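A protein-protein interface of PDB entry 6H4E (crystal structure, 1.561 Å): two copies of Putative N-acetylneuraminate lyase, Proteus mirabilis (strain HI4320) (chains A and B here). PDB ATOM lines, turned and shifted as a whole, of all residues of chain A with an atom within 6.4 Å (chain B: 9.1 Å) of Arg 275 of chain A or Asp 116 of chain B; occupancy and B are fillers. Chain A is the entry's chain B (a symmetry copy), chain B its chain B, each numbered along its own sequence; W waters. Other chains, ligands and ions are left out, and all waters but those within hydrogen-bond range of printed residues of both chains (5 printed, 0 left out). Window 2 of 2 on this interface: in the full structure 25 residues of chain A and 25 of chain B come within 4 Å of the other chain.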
ATOM      1  N   TYR A 250      -2.990   1.091  -5.801  1.00  0.00           N
ATOM      2  CA  TYR A 250      -1.571   0.834  -5.578  1.00  0.00           C
ATOM      3  C   TYR A 250      -1.212   0.486  -4.141  1.00  0.00           C
ATOM      4  O   TYR A 250      -0.051   0.143  -3.878  1.00  0.00           O
ATOM      5  CB  TYR A 250      -0.749   2.050  -6.022  1.00  0.00           C
ATOM      6  CG  TYR A 250      -0.676   2.180  -7.520  1.00  0.00           C
ATOM      7  CD1 TYR A 250      -0.122   1.164  -8.281  1.00  0.00           C
ATOM      8  CD2 TYR A 250      -1.154   3.305  -8.173  1.00  0.00           C
ATOM      9  CE1 TYR A 250      -0.048   1.256  -9.644  1.00  0.00           C
ATOM     10  CE2 TYR A 250      -1.075   3.416  -9.558  1.00  0.00           C
ATOM     11  CZ  TYR A 250      -0.515   2.380 -10.281  1.00  0.00           C
ATOM     12  OH  TYR A 250      -0.426   2.453 -11.653  1.00  0.00           O
ATOM     13  N   ALA A 254       1.789   2.407   0.332  1.00  0.00           N
ATOM     14  CA  ALA A 254       2.730   2.609  -0.766  1.00  0.00           C
ATOM     15  C   ALA A 254       2.395   3.871  -1.546  1.00  0.00           C
ATOM     16  O   ALA A 254       3.275   4.692  -1.832  1.00  0.00           O
ATOM     17  CB  ALA A 254       2.730   1.389  -1.696  1.00  0.00           C
ATOM     18  N   PRO A 270       7.516   1.420   1.487  1.00  0.00           N
ATOM     19  CA  PRO A 270       7.111   0.671   2.680  1.00  0.00           C
ATOM     20  C   PRO A 270       8.145  -0.396   3.000  1.00  0.00           C
ATOM     21  O   PRO A 270       8.960  -0.780   2.156  1.00  0.00           O
ATOM     22  CB  PRO A 270       5.775   0.031   2.282  1.00  0.00           C
ATOM     23  CG  PRO A 270       5.379   0.662   0.983  1.00  0.00           C
ATOM     24  CD  PRO A 270       6.633   1.155   0.337  1.00  0.00           C
ATOM     25  N   ARG A 271       8.107  -0.881   4.239  1.00  0.00           N
ATOM     26  CA  ARG A 271       8.892  -2.055   4.591  1.00  0.00           C
ATOM     27  C   ARG A 271       8.144  -3.321   4.201  1.00  0.00           C
ATOM     28  O   ARG A 271       6.915  -3.380   4.258  1.00  0.00           O
ATOM     29  CB  ARG A 271       9.204  -2.083   6.092  1.00  0.00           C
ATOM     30  CG  ARG A 271      10.545  -1.470   6.426  1.00  0.00           C
ATOM     31  CD  ARG A 271      10.893  -1.636   7.890  1.00  0.00           C
ATOM     32  NE  ARG A 271      12.164  -0.984   8.173  1.00  0.00           N
ATOM     33  CZ  ARG A 271      12.727  -0.952   9.378  1.00  0.00           C
ATOM     34  NH1 ARG A 271      12.131  -1.557  10.406  1.00  0.00           N
ATOM     35  NH2 ARG A 271      13.886  -0.314   9.547  1.00  0.00           N
ATOM     36  N   ARG A 272       8.899  -4.343   3.797  1.00  0.00           N
ATOM     37  CA  ARG A 272       8.339  -5.676   3.650  1.00  0.00           C
ATOM     38  C   ARG A 272       7.666  -6.076   4.967  1.00  0.00           C
ATOM     39  O   ARG A 272       8.180  -5.754   6.039  1.00  0.00           O
ATOM     40  CB  ARG A 272       9.442  -6.679   3.271  1.00  0.00           C
ATOM     41  CG  ARG A 272      10.059  -6.428   1.893  1.00  0.00           C
ATOM     42  CD  ARG A 272       9.112  -6.838   0.785  1.00  0.00           C
ATOM     43  NE  ARG A 272       9.653  -6.540  -0.542  1.00  0.00           N
ATOM     44  CZ  ARG A 272       9.022  -6.822  -1.678  1.00  0.00           C
ATOM     45  NH1 ARG A 272       7.835  -7.405  -1.646  1.00  0.00           N
ATOM     46  NH2 ARG A 272       9.584  -6.522  -2.848  1.00  0.00           N
ATOM     47  N   PRO A 273       6.539  -6.807   4.903  1.00  0.00           N
ATOM     48  CA  PRO A 273       5.928  -7.481   3.747  1.00  0.00           C
ATOM     49  C   PRO A 273       5.140  -6.618   2.774  1.00  0.00           C
ATOM     50  O   PRO A 273       4.679  -7.171   1.788  1.00  0.00           O
ATOM     51  CB  PRO A 273       4.980  -8.490   4.405  1.00  0.00           C
ATOM     52  CG  PRO A 273       4.578  -7.826   5.669  1.00  0.00           C
ATOM     53  CD  PRO A 273       5.825  -7.124   6.152  1.00  0.00           C
ATOM     54  N   LEU A 274       4.971  -5.324   3.015  1.00  0.00           N
ATOM     55  CA  LEU A 274       4.284  -4.511   2.018  1.00  0.00           C
ATOM     56  C   LEU A 274       5.130  -4.434   0.751  1.00  0.00           C
ATOM     57  O   LEU A 274       6.360  -4.408   0.804  1.00  0.00           O
ATOM     58  CB  LEU A 274       3.999  -3.108   2.553  1.00  0.00           C
ATOM     59  CG  LEU A 274       2.882  -3.011   3.587  1.00  0.00           C
ATOM     60  CD1 LEU A 274       2.880  -1.635   4.244  1.00  0.00           C
ATOM     61  CD2 LEU A 274       1.532  -3.321   2.936  1.00  0.00           C
ATOM     62  N   ARG A 275       4.454  -4.411  -0.401  1.00  0.00           N
ATOM     63  CA  ARG A 275       5.110  -4.422  -1.704  1.00  0.00           C
ATOM     64  C   ARG A 275       5.468  -3.001  -2.129  1.00  0.00           C
ATOM     65  O   ARG A 275       4.626  -2.106  -2.024  1.00  0.00           O
ATOM     66  CB  ARG A 275       4.194  -5.056  -2.738  1.00  0.00           C
ATOM     67  CG  ARG A 275       4.627  -4.889  -4.177  1.00  0.00           C
ATOM     68  CD  ARG A 275       3.469  -5.226  -5.106  1.00  0.00           C
ATOM     69  NE  ARG A 275       3.270  -6.664  -5.220  1.00  0.00           N
ATOM     70  CZ  ARG A 275       3.388  -7.346  -6.355  1.00  0.00           C
ATOM     71  NH1 ARG A 275       3.694  -6.715  -7.484  1.00  0.00           N
ATOM     72  NH2 ARG A 275       3.188  -8.658  -6.361  1.00  0.00           N
ATOM     73  N   PRO A 276       6.680  -2.763  -2.627  1.00  0.00           N
ATOM     74  CA  PRO A 276       7.019  -1.441  -3.155  1.00  0.00           C
ATOM     75  C   PRO A 276       6.441  -1.250  -4.551  1.00  0.00           C
ATOM     76  O   PRO A 276       6.066  -2.202  -5.238  1.00  0.00           O
ATOM     77  CB  PRO A 276       8.547  -1.470  -3.192  1.00  0.00           C
ATOM     78  CG  PRO A 276       8.852  -2.903  -3.528  1.00  0.00           C
ATOM     79  CD  PRO A 276       7.769  -3.732  -2.854  1.00  0.00           C
ATOM     80  N   LEU A 277       6.372   0.010  -4.963  1.00  0.00           N
ATOM     81  CA  LEU A 277       5.934   0.357  -6.309  1.00  0.00           C
ATOM     82  C   LEU A 277       7.128   0.364  -7.254  1.00  0.00           C
ATOM     83  O   LEU A 277       8.226   0.785  -6.877  1.00  0.00           O
ATOM     84  CB  LEU A 277       5.257   1.732  -6.317  1.00  0.00           C
ATOM     85  CG  LEU A 277       4.001   1.871  -5.454  1.00  0.00           C
ATOM     86  CD1 LEU A 277       3.412   3.261  -5.630  1.00  0.00           C
ATOM     87  CD2 LEU A 277       2.994   0.801  -5.827  1.00  0.00           C
ATOM     88  N   GLN A 281       4.964   2.424 -11.823  1.00  0.00           N
ATOM     89  CA  GLN A 281       3.795   2.601 -10.966  1.00  0.00           C
ATOM     90  C   GLN A 281       3.869   3.907 -10.191  1.00  0.00           C
ATOM     91  O   GLN A 281       2.854   4.591 -10.035  1.00  0.00           O
ATOM     92  CB  GLN A 281       3.662   1.419 -10.011  1.00  0.00           C
ATOM     93  CG  GLN A 281       3.358   0.118 -10.724  1.00  0.00           C
ATOM     94  CD  GLN A 281       3.366  -1.076  -9.801  1.00  0.00           C
ATOM     95  OE1 GLN A 281       4.217  -1.189  -8.918  1.00  0.00           O
ATOM     96  NE2 GLN A 281       2.433  -1.991 -10.020  1.00  0.00           N
ATOM     97  N   PRO B 106       2.451 -13.042   7.875  1.00  0.00           N
ATOM     98  CA  PRO B 106       2.111 -11.783   8.554  1.00  0.00           C
ATOM     99  C   PRO B 106       0.611 -11.542   8.516  1.00  0.00           C
ATOM    100  O   PRO B 106      -0.027 -11.671   7.467  1.00  0.00           O
ATOM    101  CB  PRO B 106       2.882 -10.728   7.748  1.00  0.00           C
ATOM    102  CG  PRO B 106       4.011 -11.489   7.109  1.00  0.00           C
ATOM    103  CD  PRO B 106       3.427 -12.847   6.790  1.00  0.00           C
ATOM    104  N   PHE B 109      -0.909  -6.408   7.914  1.00  0.00           N
ATOM    105  CA  PHE B 109      -0.843  -6.208   6.468  1.00  0.00           C
ATOM    106  C   PHE B 109      -0.743  -7.592   5.840  1.00  0.00           C
ATOM    107  O   PHE B 109       0.332  -8.193   5.806  1.00  0.00           O
ATOM    108  CB  PHE B 109       0.360  -5.352   6.083  1.00  0.00           C
ATOM    109  CG  PHE B 109       0.316  -3.932   6.594  1.00  0.00           C
ATOM    110  CD1 PHE B 109      -0.573  -3.010   6.071  1.00  0.00           C
ATOM    111  CD2 PHE B 109       1.213  -3.511   7.561  1.00  0.00           C
ATOM    112  CE1 PHE B 109      -0.583  -1.704   6.526  1.00  0.00           C
ATOM    113  CE2 PHE B 109       1.211  -2.202   8.017  1.00  0.00           C
ATOM    114  CZ  PHE B 109       0.320  -1.302   7.503  1.00  0.00           C
ATOM    115  N   LYS B 110      -1.866  -8.118   5.372  1.00  0.00           N
ATOM    116  CA  LYS B 110      -1.919  -9.496   4.898  1.00  0.00           C
ATOM    117  C   LYS B 110      -1.433  -9.572   3.457  1.00  0.00           C
ATOM    118  O   LYS B 110      -2.054  -8.966   2.577  1.00  0.00           O
ATOM    119  CB  LYS B 110      -3.347 -10.026   5.005  1.00  0.00           C
ATOM    120  CG  LYS B 110      -3.798 -10.205   6.452  1.00  0.00           C
ATOM    121  CD  LYS B 110      -5.273 -10.570   6.588  1.00  0.00           C
ATOM    122  CE  LYS B 110      -5.632 -10.732   8.068  1.00  0.00           C
ATOM    123  NZ  LYS B 110      -7.077 -10.945   8.300  1.00  0.00           N
ATOM    124  N   PRO B 111      -0.343 -10.288   3.169  1.00  0.00           N
ATOM    125  CA  PRO B 111       0.034 -10.504   1.766  1.00  0.00           C
ATOM    126  C   PRO B 111      -1.117 -11.130   0.998  1.00  0.00           C
ATOM    127  O   PRO B 111      -1.768 -12.064   1.473  1.00  0.00           O
ATOM    128  CB  PRO B 111       1.238 -11.447   1.861  1.00  0.00           C
ATOM    129  CG  PRO B 111       1.797 -11.199   3.233  1.00  0.00           C
ATOM    130  CD  PRO B 111       0.604 -10.926   4.103  1.00  0.00           C
ATOM    131  N   SER B 112      -1.388 -10.579  -0.183  1.00  0.00           N
ATOM    132  CA  SER B 112      -2.492 -11.032  -1.011  1.00  0.00           C
ATOM    133  C   SER B 112      -2.038 -11.582  -2.350  1.00  0.00           C
ATOM    134  O   SER B 112      -2.878 -12.048  -3.130  1.00  0.00           O
ATOM    135  CB  SER B 112      -3.488  -9.890  -1.246  1.00  0.00           C
ATOM    136  OG  SER B 112      -2.832  -8.780  -1.824  1.00  0.00           O
ATOM    137  N   HIS B 113      -0.746 -11.531  -2.648  1.00  0.00           N
ATOM    138  CA  HIS B 113      -0.220 -12.108  -3.873  1.00  0.00           C
ATOM    139  C   HIS B 113       0.922 -13.052  -3.533  1.00  0.00           C
ATOM    140  O   HIS B 113       1.690 -12.795  -2.601  1.00  0.00           O
ATOM    141  CB  HIS B 113       0.247 -11.015  -4.828  1.00  0.00           C
ATOM    142  CG  HIS B 113      -0.830 -10.041  -5.188  1.00  0.00           C
ATOM    143  ND1 HIS B 113      -1.884 -10.367  -6.014  1.00  0.00           N
ATOM    144  CD2 HIS B 113      -1.033  -8.757  -4.809  1.00  0.00           C
ATOM    145  CE1 HIS B 113      -2.681  -9.322  -6.142  1.00  0.00           C
ATOM    146  NE2 HIS B 113      -2.183  -8.329  -5.426  1.00  0.00           N
ATOM    147  N   VAL B 114       1.003 -14.154  -4.289  1.00  0.00           N
ATOM    148  CA  VAL B 114       2.051 -15.155  -4.087  1.00  0.00           C
ATOM    149  C   VAL B 114       3.421 -14.499  -3.969  1.00  0.00           C
ATOM    150  O   VAL B 114       4.183 -14.764  -3.028  1.00  0.00           O
ATOM    151  CB  VAL B 114       2.035 -16.182  -5.234  1.00  0.00           C
ATOM    152  CG1 VAL B 114       3.279 -17.056  -5.170  1.00  0.00           C
ATOM    153  CG2 VAL B 114       0.783 -17.029  -5.165  1.00  0.00           C
ATOM    154  N   ASP B 115       3.768 -13.646  -4.935  1.00  0.00           N
ATOM    155  CA  ASP B 115       5.133 -13.128  -4.962  1.00  0.00           C
ATOM    156  C   ASP B 115       5.442 -12.290  -3.728  1.00  0.00           C
ATOM    157  O   ASP B 115       6.600 -12.222  -3.298  1.00  0.00           O
ATOM    158  CB  ASP B 115       5.366 -12.307  -6.231  1.00  0.00           C
ATOM    159  CG  ASP B 115       5.377 -13.158  -7.477  1.00  0.00           C
ATOM    160  OD1 ASP B 115       5.479 -14.396  -7.362  1.00  0.00           O
ATOM    161  OD2 ASP B 115       5.289 -12.579  -8.581  1.00  0.00           O
ATOM    162  N   ASP B 116       4.426 -11.648  -3.147  1.00  0.00           N
ATOM    163  CA  ASP B 116       4.661 -10.830  -1.965  1.00  0.00           C
ATOM    164  C   ASP B 116       4.965 -11.695  -0.750  1.00  0.00           C
ATOM    165  O   ASP B 116       5.846 -11.365   0.052  1.00  0.00           O
ATOM    166  CB  ASP B 116       3.455  -9.929  -1.696  1.00  0.00           C
ATOM    167  CG  ASP B 116       3.179  -8.953  -2.835  1.00  0.00           C
ATOM    168  OD1 ASP B 116       4.136  -8.546  -3.529  1.00  0.00           O
ATOM    169  OD2 ASP B 116       2.003  -8.594  -3.018  1.00  0.00           O
ATOM    170  N   LEU B 117       4.250 -12.809  -0.598  1.00  0.00           N
ATOM    171  CA  LEU B 117       4.552 -13.714   0.503  1.00  0.00           C
ATOM    172  C   LEU B 117       5.898 -14.392   0.289  1.00  0.00           C
ATOM    173  O   LEU B 117       6.657 -14.595   1.242  1.00  0.00           O
ATOM    174  CB  LEU B 117       3.443 -14.756   0.640  1.00  0.00           C
ATOM    175  CG  LEU B 117       3.570 -15.742   1.803  1.00  0.00           C
ATOM    176  CD1 LEU B 117       3.566 -15.026   3.166  1.00  0.00           C
ATOM    177  CD2 LEU B 117       2.450 -16.782   1.733  1.00  0.00           C
ATOM    178  N   VAL B 118       6.211 -14.737  -0.964  1.00  0.00           N
ATOM    179  CA  VAL B 118       7.498 -15.359  -1.275  1.00  0.00           C
ATOM    180  C   VAL B 118       8.647 -14.443  -0.887  1.00  0.00           C
ATOM    181  O   VAL B 118       9.631 -14.887  -0.282  1.00  0.00           O
ATOM    182  CB  VAL B 118       7.575 -15.741  -2.764  1.00  0.00           C
ATOM    183  CG1 VAL B 118       9.014 -16.070  -3.132  1.00  0.00           C
ATOM    184  CG2 VAL B 118       6.672 -16.922  -3.049  1.00  0.00           C
ATOM    185  N   GLU B 119       8.547 -13.152  -1.222  1.00  0.00           N
ATOM    186  CA  GLU B 119       9.663 -12.252  -0.932  1.00  0.00           C
ATOM    187  C   GLU B 119       9.872 -12.084   0.568  1.00  0.00           C
ATOM    188  O   GLU B 119      11.012 -12.044   1.036  1.00  0.00           O
ATOM    189  CB  GLU B 119       9.453 -10.896  -1.601  1.00  0.00           C
ATOM    190  CG  GLU B 119      10.538  -9.860  -1.279  1.00  0.00           C
ATOM    191  CD  GLU B 119      11.926 -10.218  -1.805  1.00  0.00           C
ATOM    192  OE1 GLU B 119      12.048 -11.117  -2.661  1.00  0.00           O
ATOM    193  OE2 GLU B 119      12.907  -9.579  -1.358  1.00  0.00           O
ATOM    194  N   TYR B 120       8.790 -11.979   1.345  1.00  0.00           N
ATOM    195  CA  TYR B 120       8.936 -11.928   2.793  1.00  0.00           C
ATOM    196  C   TYR B 120       9.673 -13.161   3.310  1.00  0.00           C
ATOM    197  O   TYR B 120      10.640 -13.047   4.074  1.00  0.00           O
ATOM    198  CB  TYR B 120       7.553 -11.789   3.447  1.00  0.00           C
ATOM    199  CG  TYR B 120       7.580 -11.898   4.952  1.00  0.00           C
ATOM    200  CD1 TYR B 120       8.024 -10.841   5.741  1.00  0.00           C
ATOM    201  CD2 TYR B 120       7.177 -13.065   5.592  1.00  0.00           C
ATOM    202  CE1 TYR B 120       8.064 -10.938   7.118  1.00  0.00           C
ATOM    203  CE2 TYR B 120       7.218 -13.175   6.963  1.00  0.00           C
ATOM    204  CZ  TYR B 120       7.654 -12.115   7.729  1.00  0.00           C
ATOM    205  OH  TYR B 120       7.697 -12.223   9.104  1.00  0.00           O
ATOM    206  N   CYS B 121       9.238 -14.355   2.888  1.00  0.00           N
ATOM    207  CA  CYS B 121       9.905 -15.580   3.320  1.00  0.00           C
ATOM    208  C   CYS B 121      11.349 -15.628   2.849  1.00  0.00           C
ATOM    209  O   CYS B 121      12.221 -16.131   3.566  1.00  0.00           O
ATOM    210  CB  CYS B 121       9.153 -16.801   2.804  1.00  0.00           C
ATOM    211  SG  CYS B 121       7.546 -17.037   3.601  1.00  0.00           S
ATOM    212  N   ARG B 122      11.611 -15.136   1.633  1.00  0.00           N
ATOM    213  CA  ARG B 122      12.962 -15.185   1.080  1.00  0.00           C
ATOM    214  C   ARG B 122      13.945 -14.420   1.952  1.00  0.00           C
ATOM    215  O   ARG B 122      15.069 -14.882   2.192  1.00  0.00           O
ATOM    216  CB  ARG B 122      12.969 -14.626  -0.345  1.00  0.00           C
ATOM    217  CG  ARG B 122      14.258 -14.936  -1.114  1.00  0.00           C
ATOM    218  CD  ARG B 122      14.362 -14.111  -2.401  1.00  0.00           C
ATOM    219  NE  ARG B 122      14.424 -12.683  -2.106  1.00  0.00           N
ATOM    220  CZ  ARG B 122      15.505 -12.050  -1.659  1.00  0.00           C
ATOM    221  NH1 ARG B 122      16.638 -12.716  -1.451  1.00  0.00           N
ATOM    222  NH2 ARG B 122      15.451 -10.746  -1.406  1.00  0.00           N
ATOM    223  N   LEU B 123      13.538 -13.243   2.427  1.00  0.00           N
ATOM    224  CA  LEU B 123      14.388 -12.460   3.314  1.00  0.00           C
ATOM    225  C   LEU B 123      14.669 -13.212   4.608  1.00  0.00           C
ATOM    226  O   LEU B 123      15.810 -13.256   5.083  1.00  0.00           O
ATOM    227  CB  LEU B 123      13.724 -11.115   3.606  1.00  0.00           C
ATOM    228  CG  LEU B 123      13.593 -10.171   2.417  1.00  0.00           C
ATOM    229  CD1 LEU B 123      12.682  -9.001   2.770  1.00  0.00           C
ATOM    230  CD2 LEU B 123      14.977  -9.679   2.040  1.00  0.00           C
ATOM    231  N   TYR B 135       7.948 -22.646   5.783  1.00  0.00           N
ATOM    232  CA  TYR B 135       6.869 -21.681   5.934  1.00  0.00           C
ATOM    233  C   TYR B 135       5.839 -22.254   6.898  1.00  0.00           C
ATOM    234  O   TYR B 135       5.534 -23.446   6.865  1.00  0.00           O
ATOM    235  CB  TYR B 135       6.206 -21.346   4.589  1.00  0.00           C
ATOM    236  CG  TYR B 135       5.056 -20.361   4.736  1.00  0.00           C
ATOM    237  CD1 TYR B 135       5.280 -19.080   5.236  1.00  0.00           C
ATOM    238  CD2 TYR B 135       3.764 -20.713   4.390  1.00  0.00           C
ATOM    239  CE1 TYR B 135       4.251 -18.173   5.388  1.00  0.00           C
ATOM    240  CE2 TYR B 135       2.718 -19.817   4.544  1.00  0.00           C
ATOM    241  CZ  TYR B 135       2.968 -18.545   5.043  1.00  0.00           C
ATOM    242  OH  TYR B 135       1.931 -17.651   5.188  1.00  0.00           O
ATOM    243  N   LEU B 143      -4.710 -15.442   5.407  1.00  0.00           N
ATOM    244  CA  LEU B 143      -4.278 -15.169   4.042  1.00  0.00           C
ATOM    245  C   LEU B 143      -5.072 -16.027   3.068  1.00  0.00           C
ATOM    246  O   LEU B 143      -5.546 -17.112   3.409  1.00  0.00           O
ATOM    247  CB  LEU B 143      -2.780 -15.431   3.860  1.00  0.00           C
ATOM    248  CG  LEU B 143      -1.812 -14.768   4.843  1.00  0.00           C
ATOM    249  CD1 LEU B 143      -0.371 -14.836   4.355  1.00  0.00           C
ATOM    250  CD2 LEU B 143      -2.207 -13.326   5.092  1.00  0.00           C
ATOM    251  N   ILE B 145      -3.812 -16.946  -0.035  1.00  0.00           N
ATOM    252  CA  ILE B 145      -2.851 -17.388  -1.037  1.00  0.00           C
ATOM    253  C   ILE B 145      -2.832 -18.906  -1.067  1.00  0.00           C
ATOM    254  O   ILE B 145      -2.725 -19.553  -0.020  1.00  0.00           O
ATOM    255  CB  ILE B 145      -1.454 -16.827  -0.725  1.00  0.00           C
ATOM    256  CG1 ILE B 145      -1.494 -15.300  -0.795  1.00  0.00           C
ATOM    257  CG2 ILE B 145      -0.410 -17.416  -1.675  1.00  0.00           C
ATOM    258  CD1 ILE B 145      -0.259 -14.643  -0.226  1.00  0.00           C
ATOM    259  N   PHE B 150       2.196 -21.042  -3.789  1.00  0.00           N
ATOM    260  CA  PHE B 150       3.268 -20.447  -2.997  1.00  0.00           C
ATOM    261  C   PHE B 150       4.506 -21.331  -3.012  1.00  0.00           C
ATOM    262  O   PHE B 150       5.622 -20.853  -3.222  1.00  0.00           O
ATOM    263  CB  PHE B 150       2.810 -20.209  -1.556  1.00  0.00           C
ATOM    264  CG  PHE B 150       3.950 -19.951  -0.611  1.00  0.00           C
ATOM    265  CD1 PHE B 150       4.538 -18.701  -0.540  1.00  0.00           C
ATOM    266  CD2 PHE B 150       4.457 -20.974   0.182  1.00  0.00           C
ATOM    267  CE1 PHE B 150       5.606 -18.473   0.319  1.00  0.00           C
ATOM    268  CE2 PHE B 150       5.522 -20.754   1.038  1.00  0.00           C
ATOM    269  CZ  PHE B 150       6.093 -19.495   1.105  1.00  0.00           C
ATOM    270  N   ALA B 153       6.398 -21.279  -6.323  1.00  0.00           N
ATOM    271  CA  ALA B 153       7.122 -20.032  -6.538  1.00  0.00           C
ATOM    272  C   ALA B 153       8.285 -19.894  -5.566  1.00  0.00           C
ATOM    273  O   ALA B 153       9.378 -19.441  -5.944  1.00  0.00           O
ATOM    274  CB  ALA B 153       6.168 -18.849  -6.396  1.00  0.00           C
HETATM  275  O   HOH W   1       0.781  -6.069  -3.275  1.00  0.00           O
HETATM  276  O   HOH W   2       6.489  -8.716   0.547  1.00  0.00           O
HETATM  277  O   HOH W   3       1.602  -7.519   3.306  1.00  0.00           O
HETATM  278  O   HOH W   4       6.683  -8.485  -3.876  1.00  0.00           O
HETATM  279  O   HOH W   5      12.809  -7.028  -0.646  1.00  0.00           O
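The guanidinium group of Arg 275 of chain A lies within salt-bridge range of the side-chain carboxylate of Asp 116 of chain B, 2.7 Å away.
The side-chain carboxylate of Glu 119 of chain B is in salt-bridge range of the guanidinium group of Arg 122 of chain B (2.8 Å).
Arg 272 of chain A touches Glu 119 of chain B.
Arg 272 of chain A touches Leu 123 of chain B (CG to CD1, 3.8 Å).
Pro 106 of chain B touches Pro 273 of chain A (CB to CG, 3.95 Å).
CD1 of Phe 109 of chain B touches CD2 of Leu 274 of chain A, at 3.8 Å.
Of chain B, only Asp 116 comes within 4 Å of Arg 275 of chain A.
No residue of chain B comes within 4 Å of Pro 276 of chain A.
Of the printed residues of chain B, Arg 272 of chain A touches Glu 119 and Leu 123.
Of the printed residues of chain A, Pro 106 of chain B touches Pro 273.
Of the printed residues of chain A, Glu 119 of chain B touches Arg 272 (3.4 Å).
Arg 122 of chain B touches none of the printed residues of chain A.
Of the 11 printed residues of chain A, 4 touch a printed residue of chain B.
Hydrophobic or aromatic side chains of chain A that line the printed part of chain B: Pro 273 and Leu 274.
Along chain A the printed residues that touch a printed residue of chain B span positions 272 to 275.
Printed residues of chain B that touch a printed residue of chain A: Pro 106, Phe 109, Asp 116, Glu 119 and Leu 123.
Hydrophobic or aromatic side chains of chain B within 4 Å of the printed part of chain A: Pro 106, Phe 109 and Leu 123.
Along chain B the printed residues that touch a printed residue of chain A span positions 106 to 123.
Among the printed residues, Asp or Glu carboxylates within 4 Å of a Lys or Arg side-chain nitrogen of the other chain: Arg 275 of chain A with Asp 116 of chain B (2.7 Å).
No position is printed for both chains.
Water W4 lies within hydrogen-bond range of OD1 of Asp 116 of chain B (2.6 Å) and NH1 of Arg 272 of chain A (2.7 Å).
Water W5 bridges OE2 of Glu 119 of chain B (2.7 Å) and NE of Arg 272 of chain A (3.2 Å).
Water W2 lies within hydrogen-bond range of the backbone carbonyl oxygen of Pro 273 of chain A (2.7 Å), the backbone carbonyl oxygen of Asp 116 of chain B (2.8 Å) and the guanidinium group of Arg 272 of chain A (2.9 Å).
Water W1 lies within hydrogen-bond range of OD2 of Asp 116 of chain B (2.8 Å) and NE of Arg 275 of chain A (3.2 Å).
Water W3 lies within hydrogen-bond range of O of Phe 109 of chain B and O of Pro 273 of chain A.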
